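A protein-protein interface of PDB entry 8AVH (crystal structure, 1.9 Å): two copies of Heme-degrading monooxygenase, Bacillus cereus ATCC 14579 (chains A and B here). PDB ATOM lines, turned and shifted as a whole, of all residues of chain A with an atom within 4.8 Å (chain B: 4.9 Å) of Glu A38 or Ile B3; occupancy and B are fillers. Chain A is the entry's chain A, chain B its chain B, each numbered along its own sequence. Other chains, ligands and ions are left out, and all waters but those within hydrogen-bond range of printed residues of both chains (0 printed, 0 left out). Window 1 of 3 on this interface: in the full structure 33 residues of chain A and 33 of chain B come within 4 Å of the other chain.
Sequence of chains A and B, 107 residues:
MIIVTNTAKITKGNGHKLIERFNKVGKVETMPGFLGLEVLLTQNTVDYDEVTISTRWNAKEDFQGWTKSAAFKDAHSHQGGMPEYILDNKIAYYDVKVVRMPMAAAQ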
ATOM      1  N   GLY A  36     -22.002  -6.195  16.504  1.00  0.00           N
ATOM      2  CA  GLY A  36     -22.572  -5.460  15.387  1.00  0.00           C
ATOM      3  C   GLY A  36     -24.086  -5.539  15.368  1.00  0.00           C
ATOM      4  O   GLY A  36     -24.711  -6.495  15.816  1.00  0.00           O
ATOM      5  N   LEU A  37     -24.702  -4.488  14.827  1.00  0.00           N
ATOM      6  CA  LEU A  37     -26.136  -4.436  14.615  1.00  0.00           C
ATOM      7  C   LEU A  37     -26.377  -4.082  13.153  1.00  0.00           C
ATOM      8  O   LEU A  37     -25.679  -3.220  12.610  1.00  0.00           O
ATOM      9  CB  LEU A  37     -26.784  -3.396  15.518  1.00  0.00           C
ATOM     10  CG  LEU A  37     -28.285  -3.221  15.413  1.00  0.00           C
ATOM     11  CD1 LEU A  37     -28.789  -2.673  16.714  1.00  0.00           C
ATOM     12  CD2 LEU A  37     -28.673  -2.238  14.265  1.00  0.00           C
ATOM     13  N   GLU A  38     -27.330  -4.763  12.507  1.00  0.00           N
ATOM     14  CA  GLU A  38     -27.732  -4.380  11.155  1.00  0.00           C
ATOM     15  C   GLU A  38     -29.255  -4.350  11.048  1.00  0.00           C
ATOM     16  O   GLU A  38     -29.972  -5.086  11.733  1.00  0.00           O
ATOM     17  CB  GLU A  38     -27.125  -5.320  10.050  1.00  0.00           C
ATOM     18  CG  GLU A  38     -27.565  -6.764  10.136  1.00  0.00           C
ATOM     19  CD  GLU A  38     -26.704  -7.737   9.311  1.00  0.00           C
ATOM     20  OE1 GLU A  38     -25.858  -7.272   8.510  1.00  0.00           O
ATOM     21  OE2 GLU A  38     -26.883  -8.973   9.473  1.00  0.00           O
ATOM     22  N   VAL A  39     -29.741  -3.472  10.178  1.00  0.00           N
ATOM     23  CA  VAL A  39     -31.156  -3.378   9.853  1.00  0.00           C
ATOM     24  C   VAL A  39     -31.328  -3.780   8.390  1.00  0.00           C
ATOM     25  O   VAL A  39     -30.649  -3.237   7.504  1.00  0.00           O
ATOM     26  CB  VAL A  39     -31.692  -1.954  10.098  1.00  0.00           C
ATOM     27  CG1 VAL A  39     -33.169  -1.910   9.808  1.00  0.00           C
ATOM     28  CG2 VAL A  39     -31.413  -1.483  11.525  1.00  0.00           C
ATOM     29  N   LEU A  40     -32.230  -4.719   8.143  1.00  0.00           N
ATOM     30  CA  LEU A  40     -32.466  -5.274   6.821  1.00  0.00           C
ATOM     31  C   LEU A  40     -33.894  -4.984   6.382  1.00  0.00           C
ATOM     32  O   LEU A  40     -34.824  -5.020   7.190  1.00  0.00           O
ATOM     33  CB  LEU A  40     -32.273  -6.790   6.804  1.00  0.00           C
ATOM     34  CG  LEU A  40     -31.024  -7.299   7.523  1.00  0.00           C
ATOM     35  CD1 LEU A  40     -31.016  -8.831   7.507  1.00  0.00           C
ATOM     36  CD2 LEU A  40     -29.803  -6.778   6.809  1.00  0.00           C
ATOM     37  N   THR A  52     -35.954  -6.218   9.598  1.00  0.00           N
ATOM     38  CA  THR A  52     -35.275  -7.079  10.555  1.00  0.00           C
ATOM     39  C   THR A  52     -34.161  -6.287  11.228  1.00  0.00           C
ATOM     40  O   THR A  52     -33.323  -5.690  10.544  1.00  0.00           O
ATOM     41  CB  THR A  52     -34.685  -8.298   9.852  1.00  0.00           C
ATOM     42  OG1 THR A  52     -35.718  -9.013   9.177  1.00  0.00           O
ATOM     43  CG2 THR A  52     -33.984  -9.202  10.863  1.00  0.00           C
ATOM     44  N   ILE A  53     -34.155  -6.279  12.557  1.00  0.00           N
ATOM     45  CA  ILE A  53     -33.043  -5.758  13.339  1.00  0.00           C
ATOM     46  C   ILE A  53     -32.302  -6.958  13.899  1.00  0.00           C
ATOM     47  O   ILE A  53     -32.901  -7.814  14.558  1.00  0.00           O
ATOM     48  CB  ILE A  53     -33.504  -4.817  14.462  1.00  0.00           C
ATOM     49  CG1 ILE A  53     -34.315  -3.648  13.899  1.00  0.00           C
ATOM     50  CG2 ILE A  53     -32.286  -4.237  15.216  1.00  0.00           C
ATOM     51  CD1 ILE A  53     -35.781  -3.856  13.964  1.00  0.00           C
ATOM     52  N   SER A  54     -31.018  -7.044  13.624  1.00  0.00           N
ATOM     53  CA  SER A  54     -30.256  -8.180  14.118  1.00  0.00           C
ATOM     54  C   SER A  54     -29.021  -7.681  14.844  1.00  0.00           C
ATOM     55  O   SER A  54     -28.359  -6.744  14.385  1.00  0.00           O
ATOM     56  CB  SER A  54     -29.870  -9.118  12.983  1.00  0.00           C
ATOM     57  OG  SER A  54     -28.763  -8.609  12.303  1.00  0.00           O
ATOM     58  N   MET B   1     -24.928  -3.322  -0.247  1.00  0.00           N
ATOM     59  CA  MET B   1     -24.797  -4.616   0.416  1.00  0.00           C
ATOM     60  C   MET B   1     -26.128  -5.356   0.505  1.00  0.00           C
ATOM     61  O   MET B   1     -27.139  -4.774   0.912  1.00  0.00           O
ATOM     62  CB  MET B   1     -24.214  -4.421   1.812  1.00  0.00           C
ATOM     63  CG  MET B   1     -23.760  -5.702   2.477  1.00  0.00           C
ATOM     64  SD  MET B   1     -23.028  -5.343   4.096  1.00  0.00           S
ATOM     65  CE  MET B   1     -21.642  -4.356   3.574  1.00  0.00           C
ATOM     66  N   ILE B   2     -26.134  -6.644   0.120  1.00  0.00           N
ATOM     67  CA  ILE B   2     -27.306  -7.493   0.242  1.00  0.00           C
ATOM     68  C   ILE B   2     -26.925  -8.772   0.965  1.00  0.00           C
ATOM     69  O   ILE B   2     -25.755  -9.148   1.036  1.00  0.00           O
ATOM     70  CB  ILE B   2     -27.932  -7.855  -1.117  1.00  0.00           C
ATOM     71  CG1 ILE B   2     -27.000  -8.806  -1.874  1.00  0.00           C
ATOM     72  CG2 ILE B   2     -28.217  -6.583  -1.926  1.00  0.00           C
ATOM     73  CD1 ILE B   2     -27.680  -9.538  -3.018  1.00  0.00           C
ATOM     74  N   ILE B   3     -27.939  -9.439   1.502  1.00  0.00           N
ATOM     75  CA  ILE B   3     -27.784 -10.753   2.110  1.00  0.00           C
ATOM     76  C   ILE B   3     -28.774 -11.684   1.442  1.00  0.00           C
ATOM     77  O   ILE B   3     -29.935 -11.318   1.223  1.00  0.00           O
ATOM     78  CB  ILE B   3     -28.019 -10.724   3.639  1.00  0.00           C
ATOM     79  CG1 ILE B   3     -26.983  -9.838   4.313  1.00  0.00           C
ATOM     80  CG2 ILE B   3     -27.967 -12.154   4.204  1.00  0.00           C
ATOM     81  CD1 ILE B   3     -27.244  -9.570   5.786  1.00  0.00           C
ATOM     82  N   VAL B   4     -28.316 -12.879   1.101  1.00  0.00           N
ATOM     83  CA  VAL B   4     -29.171 -13.916   0.541  1.00  0.00           C
ATOM     84  C   VAL B   4     -29.168 -15.073   1.522  1.00  0.00           C
ATOM     85  O   VAL B   4     -28.101 -15.536   1.926  1.00  0.00           O
ATOM     86  CB  VAL B   4     -28.682 -14.372  -0.839  1.00  0.00           C
ATOM     87  CG1 VAL B   4     -29.589 -15.422  -1.377  1.00  0.00           C
ATOM     88  CG2 VAL B   4     -28.588 -13.165  -1.795  1.00  0.00           C
ATOM     89  N   THR B   5     -30.356 -15.493   1.956  1.00  0.00           N
ATOM     90  CA  THR B   5     -30.460 -16.617   2.865  1.00  0.00           C
ATOM     91  C   THR B   5     -31.214 -17.771   2.218  1.00  0.00           C
ATOM     92  O   THR B   5     -32.128 -17.583   1.406  1.00  0.00           O
ATOM     93  CB  THR B   5     -31.164 -16.245   4.192  1.00  0.00           C
ATOM     94  OG1 THR B   5     -32.546 -15.932   3.953  1.00  0.00           O
ATOM     95  CG2 THR B   5     -30.469 -15.048   4.874  1.00  0.00           C
ATOM     96  N   SER B  54     -26.362 -18.189   4.969  1.00  0.00           N
ATOM     97  CA  SER B  54     -26.414 -16.773   4.647  1.00  0.00           C
ATOM     98  C   SER B  54     -25.169 -16.411   3.848  1.00  0.00           C
ATOM     99  O   SER B  54     -24.063 -16.799   4.231  1.00  0.00           O
ATOM    100  CB  SER B  54     -26.466 -15.954   5.941  1.00  0.00           C
ATOM    101  OG  SER B  54     -26.489 -14.565   5.700  1.00  0.00           O
ATOM    102  N   THR B  55     -25.336 -15.699   2.738  1.00  0.00           N
ATOM    103  CA  THR B  55     -24.187 -15.139   2.033  1.00  0.00           C
ATOM    104  C   THR B  55     -24.400 -13.646   1.841  1.00  0.00           C
ATOM    105  O   THR B  55     -25.500 -13.199   1.504  1.00  0.00           O
ATOM    106  CB  THR B  55     -23.917 -15.800   0.667  1.00  0.00           C
ATOM    107  OG1 THR B  55     -25.076 -15.710  -0.185  1.00  0.00           O
ATOM    108  CG2 THR B  55     -23.519 -17.246   0.831  1.00  0.00           C
ATOM    109  N   ARG B  56     -23.333 -12.893   2.036  1.00  0.00           N
ATOM    110  CA  ARG B  56     -23.361 -11.441   1.998  1.00  0.00           C
ATOM    111  C   ARG B  56     -22.557 -10.973   0.791  1.00  0.00           C
ATOM    112  O   ARG B  56     -21.504 -11.538   0.487  1.00  0.00           O
ATOM    113  CB  ARG B  56     -22.791 -10.885   3.304  1.00  0.00           C
ATOM    114  CG  ARG B  56     -22.800  -9.388   3.440  1.00  0.00           C
ATOM    115  CD  ARG B  56     -22.015  -8.993   4.701  1.00  0.00           C
ATOM    116  NE  ARG B  56     -22.617  -9.584   5.899  1.00  0.00           N
ATOM    117  CZ  ARG B  56     -23.550  -8.984   6.630  1.00  0.00           C
ATOM    118  NH1 ARG B  56     -23.986  -7.774   6.329  1.00  0.00           N
ATOM    119  NH2 ARG B  56     -24.067  -9.621   7.678  1.00  0.00           N
ATOM    120  N   ALA B  92     -34.562 -16.104   0.674  1.00  0.00           N
ATOM    121  CA  ALA B  92     -34.970 -14.719   0.898  1.00  0.00           C
ATOM    122  C   ALA B  92     -33.815 -13.785   0.557  1.00  0.00           C
ATOM    123  O   ALA B  92     -32.643 -14.167   0.642  1.00  0.00           O
ATOM    124  CB  ALA B  92     -35.440 -14.502   2.344  1.00  0.00           C
ATOM    125  N   TYR B  93     -34.150 -12.567   0.147  1.00  0.00           N
ATOM    126  CA  TYR B  93     -33.157 -11.549  -0.163  1.00  0.00           C
ATOM    127  C   TYR B  93     -33.370 -10.319   0.712  1.00  0.00           C
ATOM    128  O   TYR B  93     -34.511  -9.905   0.953  1.00  0.00           O
ATOM    129  CB  TYR B  93     -33.215 -11.149  -1.637  1.00  0.00           C
ATOM    130  CG  TYR B  93     -33.238 -12.336  -2.555  1.00  0.00           C
ATOM    131  CD1 TYR B  93     -34.437 -12.922  -2.928  1.00  0.00           C
ATOM    132  CD2 TYR B  93     -32.059 -12.873  -3.055  1.00  0.00           C
ATOM    133  CE1 TYR B  93     -34.465 -14.013  -3.768  1.00  0.00           C
ATOM    134  CE2 TYR B  93     -32.079 -13.965  -3.905  1.00  0.00           C
ATOM    135  CZ  TYR B  93     -33.286 -14.528  -4.251  1.00  0.00           C
ATOM    136  OH  TYR B  93     -33.317 -15.615  -5.086  1.00  0.00           O
ATOM    137  N   TYR B  94     -32.267  -9.713   1.148  1.00  0.00           N
ATOM    138  CA  TYR B  94     -32.324  -8.583   2.058  1.00  0.00           C
ATOM    139  C   TYR B  94     -31.404  -7.475   1.579  1.00  0.00           C
ATOM    140  O   TYR B  94     -30.272  -7.728   1.158  1.00  0.00           O
ATOM    141  CB  TYR B  94     -31.939  -8.991   3.488  1.00  0.00           C
ATOM    142  CG  TYR B  94     -32.763 -10.116   4.072  1.00  0.00           C
ATOM    143  CD1 TYR B  94     -33.943  -9.853   4.764  1.00  0.00           C
ATOM    144  CD2 TYR B  94     -32.334 -11.444   3.982  1.00  0.00           C
ATOM    145  CE1 TYR B  94     -34.699 -10.887   5.330  1.00  0.00           C
ATOM    146  CE2 TYR B  94     -33.089 -12.484   4.536  1.00  0.00           C
ATOM    147  CZ  TYR B  94     -34.272 -12.190   5.210  1.00  0.00           C
ATOM    148  OH  TYR B  94     -35.017 -13.208   5.747  1.00  0.00           O
ATOM    149  N   VAL B  96     -29.280  -4.412   3.013  1.00  0.00           N
ATOM    150  CA  VAL B  96     -28.751  -3.883   4.264  1.00  0.00           C
ATOM    151  C   VAL B  96     -28.931  -2.369   4.270  1.00  0.00           C
ATOM    152  O   VAL B  96     -28.398  -1.663   3.405  1.00  0.00           O
ATOM    153  CB  VAL B  96     -27.281  -4.280   4.439  1.00  0.00           C
ATOM    154  CG1 VAL B  96     -26.711  -3.663   5.719  1.00  0.00           C
ATOM    155  CG2 VAL B  96     -27.170  -5.806   4.457  1.00  0.00           C
ATOM    156  N   VAL B  98     -28.863  -0.330   7.541  1.00  0.00           N
ATOM    157  CA  VAL B  98     -28.105   0.308   8.607  1.00  0.00           C
ATOM    158  C   VAL B  98     -27.075  -0.697   9.100  1.00  0.00           C
ATOM    159  O   VAL B  98     -27.388  -1.885   9.229  1.00  0.00           O
ATOM    160  CB  VAL B  98     -29.000   0.733   9.796  1.00  0.00           C
ATOM    161  CG1 VAL B  98     -28.153   1.411  10.887  1.00  0.00           C
ATOM    162  CG2 VAL B  98     -30.156   1.631   9.340  1.00  0.00           C
ATOM    163  N   VAL B  99     -25.855  -0.229   9.361  1.00  0.00           N
ATOM    164  CA  VAL B  99     -24.833  -1.046  10.014  1.00  0.00           C
ATOM    165  C   VAL B  99     -24.227  -0.248  11.153  1.00  0.00           C
ATOM    166  O   VAL B  99     -23.609   0.799  10.920  1.00  0.00           O
ATOM    167  CB  VAL B  99     -23.730  -1.484   9.044  1.00  0.00           C
ATOM    168  CG1 VAL B  99     -22.657  -2.253   9.825  1.00  0.00           C
ATOM    169  CG2 VAL B  99     -24.318  -2.319   7.922  1.00  0.00           C
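Among the printed residues, merely in contact across the chains: Glu A38 with Val B98 (3.2 Å), Leu A37 with Val B99 (3.5 Å), Leu A40 with Val B96 (3.7 Å), Glu A38 with Ile B3 (3.8 Å), Val A39 with Val B96 (3.8 Å), Leu A40 with Ile B3 (3.9 Å) and Leu A40 with Tyr B94 (3.99 Å).
Position printed for both chains: 54.
The backbone NH (N) of Val B96 lies within hydrogen-bond range of the backbone carbonyl oxygen (O) of Met B1, 3.0 Å away. The backbone NH (N) of Tyr B94 lies within hydrogen-bond range of the backbone carbonyl oxygen (O) of Ile B3. The backbone NH (N) of Leu A40 lies within hydrogen-bond range of the backbone carbonyl oxygen (O) of Thr A52. The backbone NH of Ser A54 sits at hydrogen-bond distance from the backbone carbonyl oxygen of Glu A38 (2.9 Å). The guanidinium group of Arg B56 lies within hydrogen-bond range of the side-chain sulfur of Met B1 (3.4 Å).
Of chain B, only Ile B3, Arg B56 and Val B98 come within 4 Å of Glu A38. Printed residues of chain B within 4 Å of Leu A40: Ile B3 (3.9 Å), Tyr B94 (3.99 Å) and Val B96 (3.7 Å). Ile B3 touches just these residues of chain A: Glu A38 (3.8 Å) and Leu A40 (3.9 Å). Val B4 touches none of the printed residues of chain A. Thr B55 touches none of the printed residues of chain A. Printed residues of chain A within 4 Å of Tyr B94: Leu A40 (3.99 Å). Of the printed residues of chain A, Val B99 touches Leu A37 (3.5 Å). The nearest printed residue of chain A that does not touch Ile B3 is Ser A54 (6.8 Å).
OE1 of Glu A38 is in salt-bridge range of NH1 of Arg B56, 2.9 Å away. The backbone NH (N) of Val A39 lies within hydrogen-bond range of the backbone carbonyl oxygen (O) of Val B98 (3.0 Å).
Of the 8 printed residues of chain A, 4 touch a printed residue of chain B. Hydrophobic or aromatic side chains of chain A that line the printed part of chain B: Val A39 and Leu A40. Among the printed residues, 9 pairs touch across the chains. Among the printed residues, Asp or Glu carboxylates within 4 Å of a Lys or Arg side-chain nitrogen of the other chain: Glu A38 with Arg B56.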
